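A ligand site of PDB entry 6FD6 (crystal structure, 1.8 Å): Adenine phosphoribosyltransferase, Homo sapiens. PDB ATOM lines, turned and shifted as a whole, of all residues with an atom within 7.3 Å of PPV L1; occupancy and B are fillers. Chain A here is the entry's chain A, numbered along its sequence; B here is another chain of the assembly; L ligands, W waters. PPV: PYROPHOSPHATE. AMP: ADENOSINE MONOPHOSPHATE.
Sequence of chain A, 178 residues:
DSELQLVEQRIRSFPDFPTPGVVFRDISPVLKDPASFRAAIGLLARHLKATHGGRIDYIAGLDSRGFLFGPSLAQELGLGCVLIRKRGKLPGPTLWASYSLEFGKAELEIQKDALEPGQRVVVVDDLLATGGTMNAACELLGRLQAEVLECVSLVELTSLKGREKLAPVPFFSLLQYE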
ATOM      1  N   PHE A  24       5.828  -5.621  -7.340  1.00  0.00           N
ATOM      2  CA  PHE A  24       7.216  -6.031  -7.540  1.00  0.00           C
ATOM      3  C   PHE A  24       7.724  -5.504  -8.861  1.00  0.00           C
ATOM      4  O   PHE A  24       7.085  -5.695  -9.890  1.00  0.00           O
ATOM      5  CB  PHE A  24       7.326  -7.553  -7.500  1.00  0.00           C
ATOM      6  CG  PHE A  24       8.743  -8.049  -7.470  1.00  0.00           C
ATOM      7  CD1 PHE A  24       9.455  -8.209  -8.627  1.00  0.00           C
ATOM      8  CD2 PHE A  24       9.356  -8.350  -6.262  1.00  0.00           C
ATOM      9  CE1 PHE A  24      10.761  -8.655  -8.599  1.00  0.00           C
ATOM     10  CE2 PHE A  24      10.660  -8.802  -6.210  1.00  0.00           C
ATOM     11  CZ  PHE A  24      11.361  -8.962  -7.394  1.00  0.00           C
ATOM     12  N   LEU A  62      25.716  -4.675  -4.102  1.00  0.00           N
ATOM     13  CA  LEU A  62      24.989  -5.358  -3.047  1.00  0.00           C
ATOM     14  C   LEU A  62      24.366  -6.689  -3.472  1.00  0.00           C
ATOM     15  O   LEU A  62      23.653  -6.765  -4.478  1.00  0.00           O
ATOM     16  CB  LEU A  62      23.862  -4.468  -2.518  1.00  0.00           C
ATOM     17  CG  LEU A  62      24.250  -3.083  -2.077  1.00  0.00           C
ATOM     18  CD1 LEU A  62      23.085  -2.501  -1.302  1.00  0.00           C
ATOM     19  CD2 LEU A  62      25.511  -3.083  -1.231  1.00  0.00           C
ATOM     20  N   ASP A  63      24.635  -7.713  -2.676  1.00  0.00           N
ATOM     21  CA  ASP A  63      24.072  -9.062  -2.837  1.00  0.00           C
ATOM     22  C   ASP A  63      22.536  -8.927  -2.756  1.00  0.00           C
ATOM     23  O   ASP A  63      22.051  -8.307  -1.826  1.00  0.00           O
ATOM     24  CB  ASP A  63      24.627  -9.875  -1.657  1.00  0.00           C
ATOM     25  CG  ASP A  63      24.466 -11.379  -1.793  1.00  0.00           C
ATOM     26  OD1 ASP A  63      23.910 -11.873  -2.811  1.00  0.00           O
ATOM     27  OD2 ASP A  63      24.918 -12.063  -0.853  1.00  0.00           O
ATOM     28  N   SER A  64      21.749  -9.457  -3.693  1.00  0.00           N
ATOM     29  CA  SER A  64      22.225 -10.230  -4.833  1.00  0.00           C
ATOM     30  C   SER A  64      22.010  -9.496  -6.160  1.00  0.00           C
ATOM     31  O   SER A  64      22.796  -9.632  -7.096  1.00  0.00           O
ATOM     32  CB  SER A  64      21.516 -11.592  -4.876  1.00  0.00           C
ATOM     33  OG  SER A  64      21.935 -12.438  -3.804  1.00  0.00           O
ATOM     34  N   ARG A  65      20.921  -8.742  -6.277  1.00  0.00           N
ATOM     35  CA  ARG A  65      20.621  -8.143  -7.580  1.00  0.00           C
ATOM     36  C   ARG A  65      21.578  -7.017  -7.946  1.00  0.00           C
ATOM     37  O   ARG A  65      21.757  -6.706  -9.127  1.00  0.00           O
ATOM     38  CB  ARG A  65      19.167  -7.704  -7.650  1.00  0.00           C
ATOM     39  CG  ARG A  65      18.226  -8.878  -7.866  1.00  0.00           C
ATOM     40  CD  ARG A  65      16.766  -8.469  -7.805  1.00  0.00           C
ATOM     41  NE  ARG A  65      16.254  -8.644  -6.448  1.00  0.00           N
ATOM     42  CZ  ARG A  65      15.229  -7.982  -5.938  1.00  0.00           C
ATOM     43  NH1 ARG A  65      14.616  -7.056  -6.662  1.00  0.00           N
ATOM     44  NH2 ARG A  65      14.830  -8.227  -4.694  1.00  0.00           N
ATOM     45  N   GLY A  66      22.215  -6.419  -6.943  1.00  0.00           N
ATOM     46  CA  GLY A  66      23.234  -5.409  -7.236  1.00  0.00           C
ATOM     47  C   GLY A  66      24.456  -6.010  -7.905  1.00  0.00           C
ATOM     48  O   GLY A  66      25.226  -5.315  -8.567  1.00  0.00           O
ATOM     49  N   LYS A  86      25.069 -10.874   1.975  1.00  0.00           N
ATOM     50  CA  LYS A  86      24.358 -11.440   3.109  1.00  0.00           C
ATOM     51  C   LYS A  86      25.350 -12.137   4.045  1.00  0.00           C
ATOM     52  O   LYS A  86      26.286 -12.825   3.600  1.00  0.00           O
ATOM     53  CB  LYS A  86      23.300 -12.418   2.614  1.00  0.00           C
ATOM     54  CG  LYS A  86      22.314 -11.781   1.667  1.00  0.00           C
ATOM     55  CD  LYS A  86      21.745 -10.492   2.250  1.00  0.00           C
ATOM     56  CE  LYS A  86      20.503 -10.016   1.507  1.00  0.00           C
ATOM     57  NZ  LYS A  86      20.795  -9.025   0.442  1.00  0.00           N
ATOM     58  N   TYR A  99      19.846  -5.100   9.980  1.00  0.00           N
ATOM     59  CA  TYR A  99      18.917  -4.114   9.486  1.00  0.00           C
ATOM     60  C   TYR A  99      17.583  -4.840   9.418  1.00  0.00           C
ATOM     61  O   TYR A  99      17.549  -6.076   9.509  1.00  0.00           O
ATOM     62  CB  TYR A  99      19.384  -3.564   8.120  1.00  0.00           C
ATOM     63  CG  TYR A  99      19.391  -4.565   6.992  1.00  0.00           C
ATOM     64  CD1 TYR A  99      20.398  -5.519   6.888  1.00  0.00           C
ATOM     65  CD2 TYR A  99      18.380  -4.574   6.041  1.00  0.00           C
ATOM     66  CE1 TYR A  99      20.401  -6.458   5.861  1.00  0.00           C
ATOM     67  CE2 TYR A  99      18.379  -5.500   5.008  1.00  0.00           C
ATOM     68  CZ  TYR A  99      19.380  -6.436   4.929  1.00  0.00           C
ATOM     69  OH  TYR A  99      19.356  -7.359   3.921  1.00  0.00           O
ATOM     70  N   LEU A 101      14.304  -6.231   7.640  1.00  0.00           N
ATOM     71  CA  LEU A 101      13.895  -6.683   6.337  1.00  0.00           C
ATOM     72  C   LEU A 101      12.549  -7.392   6.472  1.00  0.00           C
ATOM     73  O   LEU A 101      12.407  -8.344   7.245  1.00  0.00           O
ATOM     74  CB  LEU A 101      14.937  -7.625   5.727  1.00  0.00           C
ATOM     75  CG  LEU A 101      14.639  -8.208   4.342  1.00  0.00           C
ATOM     76  CD1 LEU A 101      14.604  -7.114   3.275  1.00  0.00           C
ATOM     77  CD2 LEU A 101      15.664  -9.276   4.003  1.00  0.00           C
ATOM     78  N   GLU A 102      11.561  -6.898   5.730  1.00  0.00           N
ATOM     79  CA  GLU A 102      10.209  -7.435   5.815  1.00  0.00           C
ATOM     80  C   GLU A 102       9.780  -7.518   7.285  1.00  0.00           C
ATOM     81  O   GLU A 102       9.689  -6.489   7.945  1.00  0.00           O
ATOM     82  CB  GLU A 102      10.136  -8.787   5.101  1.00  0.00           C
ATOM     83  CG  GLU A 102      10.470  -8.663   3.616  1.00  0.00           C
ATOM     84  CD  GLU A 102      10.471  -9.995   2.889  1.00  0.00           C
ATOM     85  OE1 GLU A 102      10.920 -11.003   3.478  1.00  0.00           O
ATOM     86  OE2 GLU A 102      10.029 -10.032   1.725  1.00  0.00           O
ATOM     87  N   ALA A 106      17.791  -9.009   9.112  1.00  0.00           N
ATOM     88  CA  ALA A 106      18.757  -9.690   8.261  1.00  0.00           C
ATOM     89  C   ALA A 106      20.095  -9.004   8.500  1.00  0.00           C
ATOM     90  O   ALA A 106      20.131  -7.955   9.157  1.00  0.00           O
ATOM     91  CB  ALA A 106      18.364  -9.586   6.799  1.00  0.00           C
ATOM     92  N   LEU A 108      24.001  -7.859   6.697  1.00  0.00           N
ATOM     93  CA  LEU A 108      24.959  -7.743   5.607  1.00  0.00           C
ATOM     94  C   LEU A 108      26.360  -7.771   6.202  1.00  0.00           C
ATOM     95  O   LEU A 108      26.557  -7.496   7.395  1.00  0.00           O
ATOM     96  CB  LEU A 108      24.778  -6.443   4.841  1.00  0.00           C
ATOM     97  CG  LEU A 108      23.491  -6.234   4.038  1.00  0.00           C
ATOM     98  CD1 LEU A 108      23.573  -4.869   3.383  1.00  0.00           C
ATOM     99  CD2 LEU A 108      23.286  -7.314   2.991  1.00  0.00           C
ATOM    100  N   ASP A 125      22.654  -0.847  -6.183  1.00  0.00           N
ATOM    101  CA  ASP A 125      21.708  -1.951  -6.056  1.00  0.00           C
ATOM    102  C   ASP A 125      20.684  -1.756  -7.158  1.00  0.00           C
ATOM    103  O   ASP A 125      20.690  -0.728  -7.840  1.00  0.00           O
ATOM    104  CB  ASP A 125      21.035  -1.940  -4.688  1.00  0.00           C
ATOM    105  CG  ASP A 125      20.521  -3.313  -4.261  1.00  0.00           C
ATOM    106  OD1 ASP A 125      20.607  -4.284  -5.055  1.00  0.00           O
ATOM    107  OD2 ASP A 125      20.053  -3.406  -3.095  1.00  0.00           O
ATOM    108  N   ASP A 126      19.830  -2.751  -7.392  1.00  0.00           N
ATOM    109  CA  ASP A 126      18.854  -2.614  -8.446  1.00  0.00           C
ATOM    110  C   ASP A 126      17.745  -1.636  -8.074  1.00  0.00           C
ATOM    111  O   ASP A 126      17.295  -0.845  -8.893  1.00  0.00           O
ATOM    112  CB  ASP A 126      18.287  -3.983  -8.870  1.00  0.00           C
ATOM    113  CG  ASP A 126      17.391  -4.627  -7.847  1.00  0.00           C
ATOM    114  OD1 ASP A 126      17.630  -4.510  -6.619  1.00  0.00           O
ATOM    115  OD2 ASP A 126      16.420  -5.311  -8.275  1.00  0.00           O
ATOM    116  N   LEU A 127      17.316  -1.688  -6.817  1.00  0.00           N
ATOM    117  CA  LEU A 127      16.151  -0.921  -6.396  1.00  0.00           C
ATOM    118  C   LEU A 127      16.303  -0.454  -4.971  1.00  0.00           C
ATOM    119  O   LEU A 127      16.805  -1.186  -4.119  1.00  0.00           O
ATOM    120  CB  LEU A 127      14.887  -1.792  -6.545  1.00  0.00           C
ATOM    121  CG  LEU A 127      13.548  -1.167  -6.119  1.00  0.00           C
ATOM    122  CD1 LEU A 127      12.426  -1.678  -6.987  1.00  0.00           C
ATOM    123  CD2 LEU A 127      13.276  -1.488  -4.644  1.00  0.00           C
ATOM    124  N   THR A 133      18.518  -1.694   3.349  1.00  0.00           N
ATOM    125  CA  THR A 133      19.651  -2.430   2.758  1.00  0.00           C
ATOM    126  C   THR A 133      20.802  -1.485   2.437  1.00  0.00           C
ATOM    127  O   THR A 133      21.944  -1.714   2.856  1.00  0.00           O
ATOM    128  CB  THR A 133      19.176  -3.189   1.501  1.00  0.00           C
ATOM    129  OG1 THR A 133      18.098  -4.051   1.856  1.00  0.00           O
ATOM    130  CG2 THR A 133      20.289  -4.060   0.849  1.00  0.00           C
ATOM    131  N   ASP B  63      22.374 -17.481  -9.479  1.00  0.00           N
ATOM    132  CA  ASP B  63      22.301 -16.738  -8.222  1.00  0.00           C
ATOM    133  C   ASP B  63      23.227 -17.441  -7.230  1.00  0.00           C
ATOM    134  O   ASP B  63      23.139 -18.658  -7.110  1.00  0.00           O
ATOM    135  CB  ASP B  63      20.832 -16.868  -7.814  1.00  0.00           C
ATOM    136  CG  ASP B  63      20.433 -16.004  -6.642  1.00  0.00           C
ATOM    137  OD1 ASP B  63      21.275 -15.309  -6.043  1.00  0.00           O
ATOM    138  OD2 ASP B  63      19.233 -16.037  -6.322  1.00  0.00           O
ATOM    139  N   SER B  64      24.144 -16.736  -6.562  1.00  0.00           N
ATOM    140  CA  SER B  64      24.286 -15.284  -6.662  1.00  0.00           C
ATOM    141  C   SER B  64      25.609 -14.873  -7.322  1.00  0.00           C
ATOM    142  O   SER B  64      25.688 -13.837  -7.956  1.00  0.00           O
ATOM    143  CB  SER B  64      24.205 -14.639  -5.274  1.00  0.00           C
ATOM    144  OG  SER B  64      22.994 -14.966  -4.612  1.00  0.00           O
ATOM    145  N   PHE B  67      25.784 -14.124 -11.029  1.00  0.00           N
ATOM    146  CA  PHE B  67      25.266 -12.815 -11.399  1.00  0.00           C
ATOM    147  C   PHE B  67      26.414 -11.834 -11.643  1.00  0.00           C
ATOM    148  O   PHE B  67      26.254 -10.845 -12.352  1.00  0.00           O
ATOM    149  CB  PHE B  67      24.402 -12.245 -10.269  1.00  0.00           C
ATOM    150  CG  PHE B  67      23.026 -12.845 -10.160  1.00  0.00           C
ATOM    151  CD1 PHE B  67      22.644 -13.903 -10.956  1.00  0.00           C
ATOM    152  CD2 PHE B  67      22.135 -12.350  -9.219  1.00  0.00           C
ATOM    153  CE1 PHE B  67      21.368 -14.448 -10.840  1.00  0.00           C
ATOM    154  CE2 PHE B  67      20.864 -12.894  -9.089  1.00  0.00           C
ATOM    155  CZ  PHE B  67      20.480 -13.934  -9.914  1.00  0.00           C
ATOM    156  N   ARG B  85      17.431 -18.305 -10.205  1.00  0.00           N
ATOM    157  CA  ARG B  85      17.521 -17.768  -8.862  1.00  0.00           C
ATOM    158  C   ARG B  85      17.306 -18.805  -7.796  1.00  0.00           C
ATOM    159  O   ARG B  85      16.741 -19.866  -8.043  1.00  0.00           O
ATOM    160  CB  ARG B  85      16.506 -16.651  -8.669  1.00  0.00           C
ATOM    161  CG  ARG B  85      16.798 -15.412  -9.505  1.00  0.00           C
ATOM    162  CD  ARG B  85      16.601 -14.135  -8.710  1.00  0.00           C
ATOM    163  NE  ARG B  85      17.470 -14.134  -7.530  1.00  0.00           N
ATOM    164  CZ  ARG B  85      17.532 -13.157  -6.626  1.00  0.00           C
ATOM    165  NH1 ARG B  85      16.776 -12.076  -6.739  1.00  0.00           N
ATOM    166  NH2 ARG B  85      18.352 -13.279  -5.580  1.00  0.00           N
ATOM    167  N   LYS B  86      17.727 -18.494  -6.576  1.00  0.00           N
ATOM    168  CA  LYS B  86      17.317 -19.297  -5.439  1.00  0.00           C
ATOM    169  C   LYS B  86      15.792 -19.183  -5.325  1.00  0.00           C
ATOM    170  O   LYS B  86      15.215 -18.125  -5.554  1.00  0.00           O
ATOM    171  CB  LYS B  86      18.031 -18.800  -4.171  1.00  0.00           C
ATOM    172  CG  LYS B  86      19.547 -18.817  -4.265  1.00  0.00           C
ATOM    173  CD  LYS B  86      20.058 -20.250  -4.395  1.00  0.00           C
ATOM    174  CE  LYS B  86      21.560 -20.323  -4.666  1.00  0.00           C
ATOM    175  NZ  LYS B  86      22.384 -19.970  -3.488  1.00  0.00           N
ATOM    176  N   LYS B  89      12.450 -15.937  -4.984  1.00  0.00           N
ATOM    177  CA  LYS B  89      12.889 -14.590  -5.306  1.00  0.00           C
ATOM    178  C   LYS B  89      12.219 -13.993  -6.557  1.00  0.00           C
ATOM    179  O   LYS B  89      12.213 -12.776  -6.747  1.00  0.00           O
ATOM    180  CB  LYS B  89      14.400 -14.613  -5.512  1.00  0.00           C
ATOM    181  CG  LYS B  89      15.176 -15.169  -4.325  1.00  0.00           C
ATOM    182  CD  LYS B  89      15.562 -14.100  -3.318  1.00  0.00           C
ATOM    183  CE  LYS B  89      16.403 -14.684  -2.186  1.00  0.00           C
ATOM    184  NZ  LYS B  89      17.452 -13.748  -1.703  1.00  0.00           N
HETATM  185  O11 PPV L   1      16.958  -8.736   0.027  1.00  0.00           O
HETATM  186  P1  PPV L   1      16.428  -8.718  -1.391  1.00  0.00           P
HETATM  187  O21 PPV L   1      16.903  -7.511  -2.191  1.00  0.00           O
HETATM  188  O31 PPV L   1      14.942  -8.984  -1.447  1.00  0.00           O
HETATM  189  OPP PPV L   1      17.066 -10.059  -2.030  1.00  0.00           O
HETATM  190  P2  PPV L   1      17.800 -10.330  -3.455  1.00  0.00           P
HETATM  191  O12 PPV L   1      18.791  -9.212  -3.706  1.00  0.00           O
HETATM  192  O22 PPV L   1      18.403 -11.700  -3.157  1.00  0.00           O
HETATM  193  O32 PPV L   1      16.691 -10.392  -4.459  1.00  0.00           O
HETATM  194  P   AMP L   2      14.993  -1.885   1.094  1.00  0.00           P
HETATM  195  O1P AMP L   2      13.601  -1.854   1.679  1.00  0.00           O
HETATM  196  O2P AMP L   2      15.373  -0.650   0.338  1.00  0.00           O
HETATM  197  O3P AMP L   2      16.067  -2.372   2.046  1.00  0.00           O
HETATM  198  O5' AMP L   2      14.821  -3.098   0.071  1.00  0.00           O
HETATM  199  C5' AMP L   2      15.655  -3.089  -1.063  1.00  0.00           C
HETATM  200  C4' AMP L   2      16.023  -4.515  -1.417  1.00  0.00           C
HETATM  201  O4' AMP L   2      14.884  -5.374  -1.546  1.00  0.00           O
HETATM  202  C3' AMP L   2      16.663  -4.363  -2.763  1.00  0.00           C
HETATM  203  O3' AMP L   2      17.808  -5.223  -2.791  1.00  0.00           O
HETATM  204  C2' AMP L   2      15.533  -4.696  -3.716  1.00  0.00           C
HETATM  205  O2' AMP L   2      16.052  -5.505  -4.760  1.00  0.00           O
HETATM  206  C1' AMP L   2      14.442  -5.433  -2.915  1.00  0.00           C
HETATM  207  N9  AMP L   2      13.063  -4.858  -3.103  1.00  0.00           N
HETATM  208  C8  AMP L   2      12.357  -4.151  -2.186  1.00  0.00           C
HETATM  209  N7  AMP L   2      11.138  -3.764  -2.665  1.00  0.00           N
HETATM  210  C5  AMP L   2      11.037  -4.241  -3.943  1.00  0.00           C
HETATM  211  C6  AMP L   2      10.036  -4.201  -5.041  1.00  0.00           C
HETATM  212  N6  AMP L   2       8.849  -3.567  -4.886  1.00  0.00           N
HETATM  213  N1  AMP L   2      10.331  -4.808  -6.216  1.00  0.00           N
HETATM  214  C2  AMP L   2      11.505  -5.450  -6.396  1.00  0.00           C
HETATM  215  N3  AMP L   2      12.461  -5.528  -5.448  1.00  0.00           N
HETATM  216  C4  AMP L   2      12.313  -4.957  -4.217  1.00  0.00           C
HETATM  217  O   HOH W   1      12.293  -7.994  -2.952  1.00  0.00           O
HETATM  218  O   HOH W   2      18.142  -6.844   1.416  1.00  0.00           O
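Water W2 lies within hydrogen-bond range of an oxygen (O11) of PPV L1 (2.6 Å), the side-chain hydroxyl (OG1) of Thr 133 (2.8 Å) and the side-chain hydroxyl (OH) of Tyr 99 (2.8 Å).
Water W1 lies within hydrogen-bond range of NH2 of Arg 65 (3.1 Å) and O31 of PPV L1 (3.2 Å).
NH1 of Arg 65 lies within salt-bridge range of OD2 of Asp 126, 3.0 Å away.
NZ of Lys 86 of chain A is in hydrogen-bond range of O of Asp 63 of chain A (2.7 Å).
The side-chain carboxylate (OD2) of Asp 63 of chain B is in salt-bridge range of the guanidinium group (NE) of Arg 85 of chain B (2.9 Å).
OG of Ser 64 of chain B lies within hydrogen-bond range of OG of Ser 64 of chain A (2.9 Å).
An oxygen (O32) of PPV L1 lies within salt-bridge range of the guanidinium group (NH1) of Arg 85 of chain B, at 2.8 Å.
N of Arg 65 sits at hydrogen-bond distance from O12 of PPV L1 (3.4 Å).
The guanidinium group (NH1) of Arg 65 is in hydrogen-bond range of an oxygen (O2') of AMP L2 (2.8 Å).
O3P of AMP L2 lies within hydrogen-bond range of OG1 of Thr 133 (2.6 Å).
O3' of AMP L2 sits at hydrogen-bond distance from OD2 of Asp 125 (2.9 Å).
The side-chain amino group (NZ) of Lys 89 of chain B is in salt-bridge range of an oxygen (O22) of PPV L1 (2.7 Å).
An oxygen (O3P) of AMP L2 lies within hydrogen-bond range of the backbone NH (N) of Thr 133, at 2.9 Å.
The side-chain carboxylate (OD1) of Asp 126 sits at hydrogen-bond distance from an oxygen (O2') of AMP L2, at 2.6 Å.
O11 of PPV L1 is in salt-bridge range of NZ of Lys 86 of chain A, at 3.9 Å.
N of Ser 64 of chain A sits at hydrogen-bond distance from O12 of PPV L1, 3.0 Å away.
The guanidinium group (NE) of Arg 65 lies within salt-bridge range of an oxygen (O32) of PPV L1 (2.7 Å).
Merely in contact with PPV L1: Asp 63 of chain A.
Six residues have an atom within 4 Å of PPV L1: Asp 63 of chain A, Ser 64 of chain A, Arg 65, Lys 86 of chain A, Arg 85 of chain B and Lys 89 of chain B.
An oxygen (O3') of AMP L2 sits at hydrogen-bond distance from an oxygen (O21) of PPV L1 (2.5 Å).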
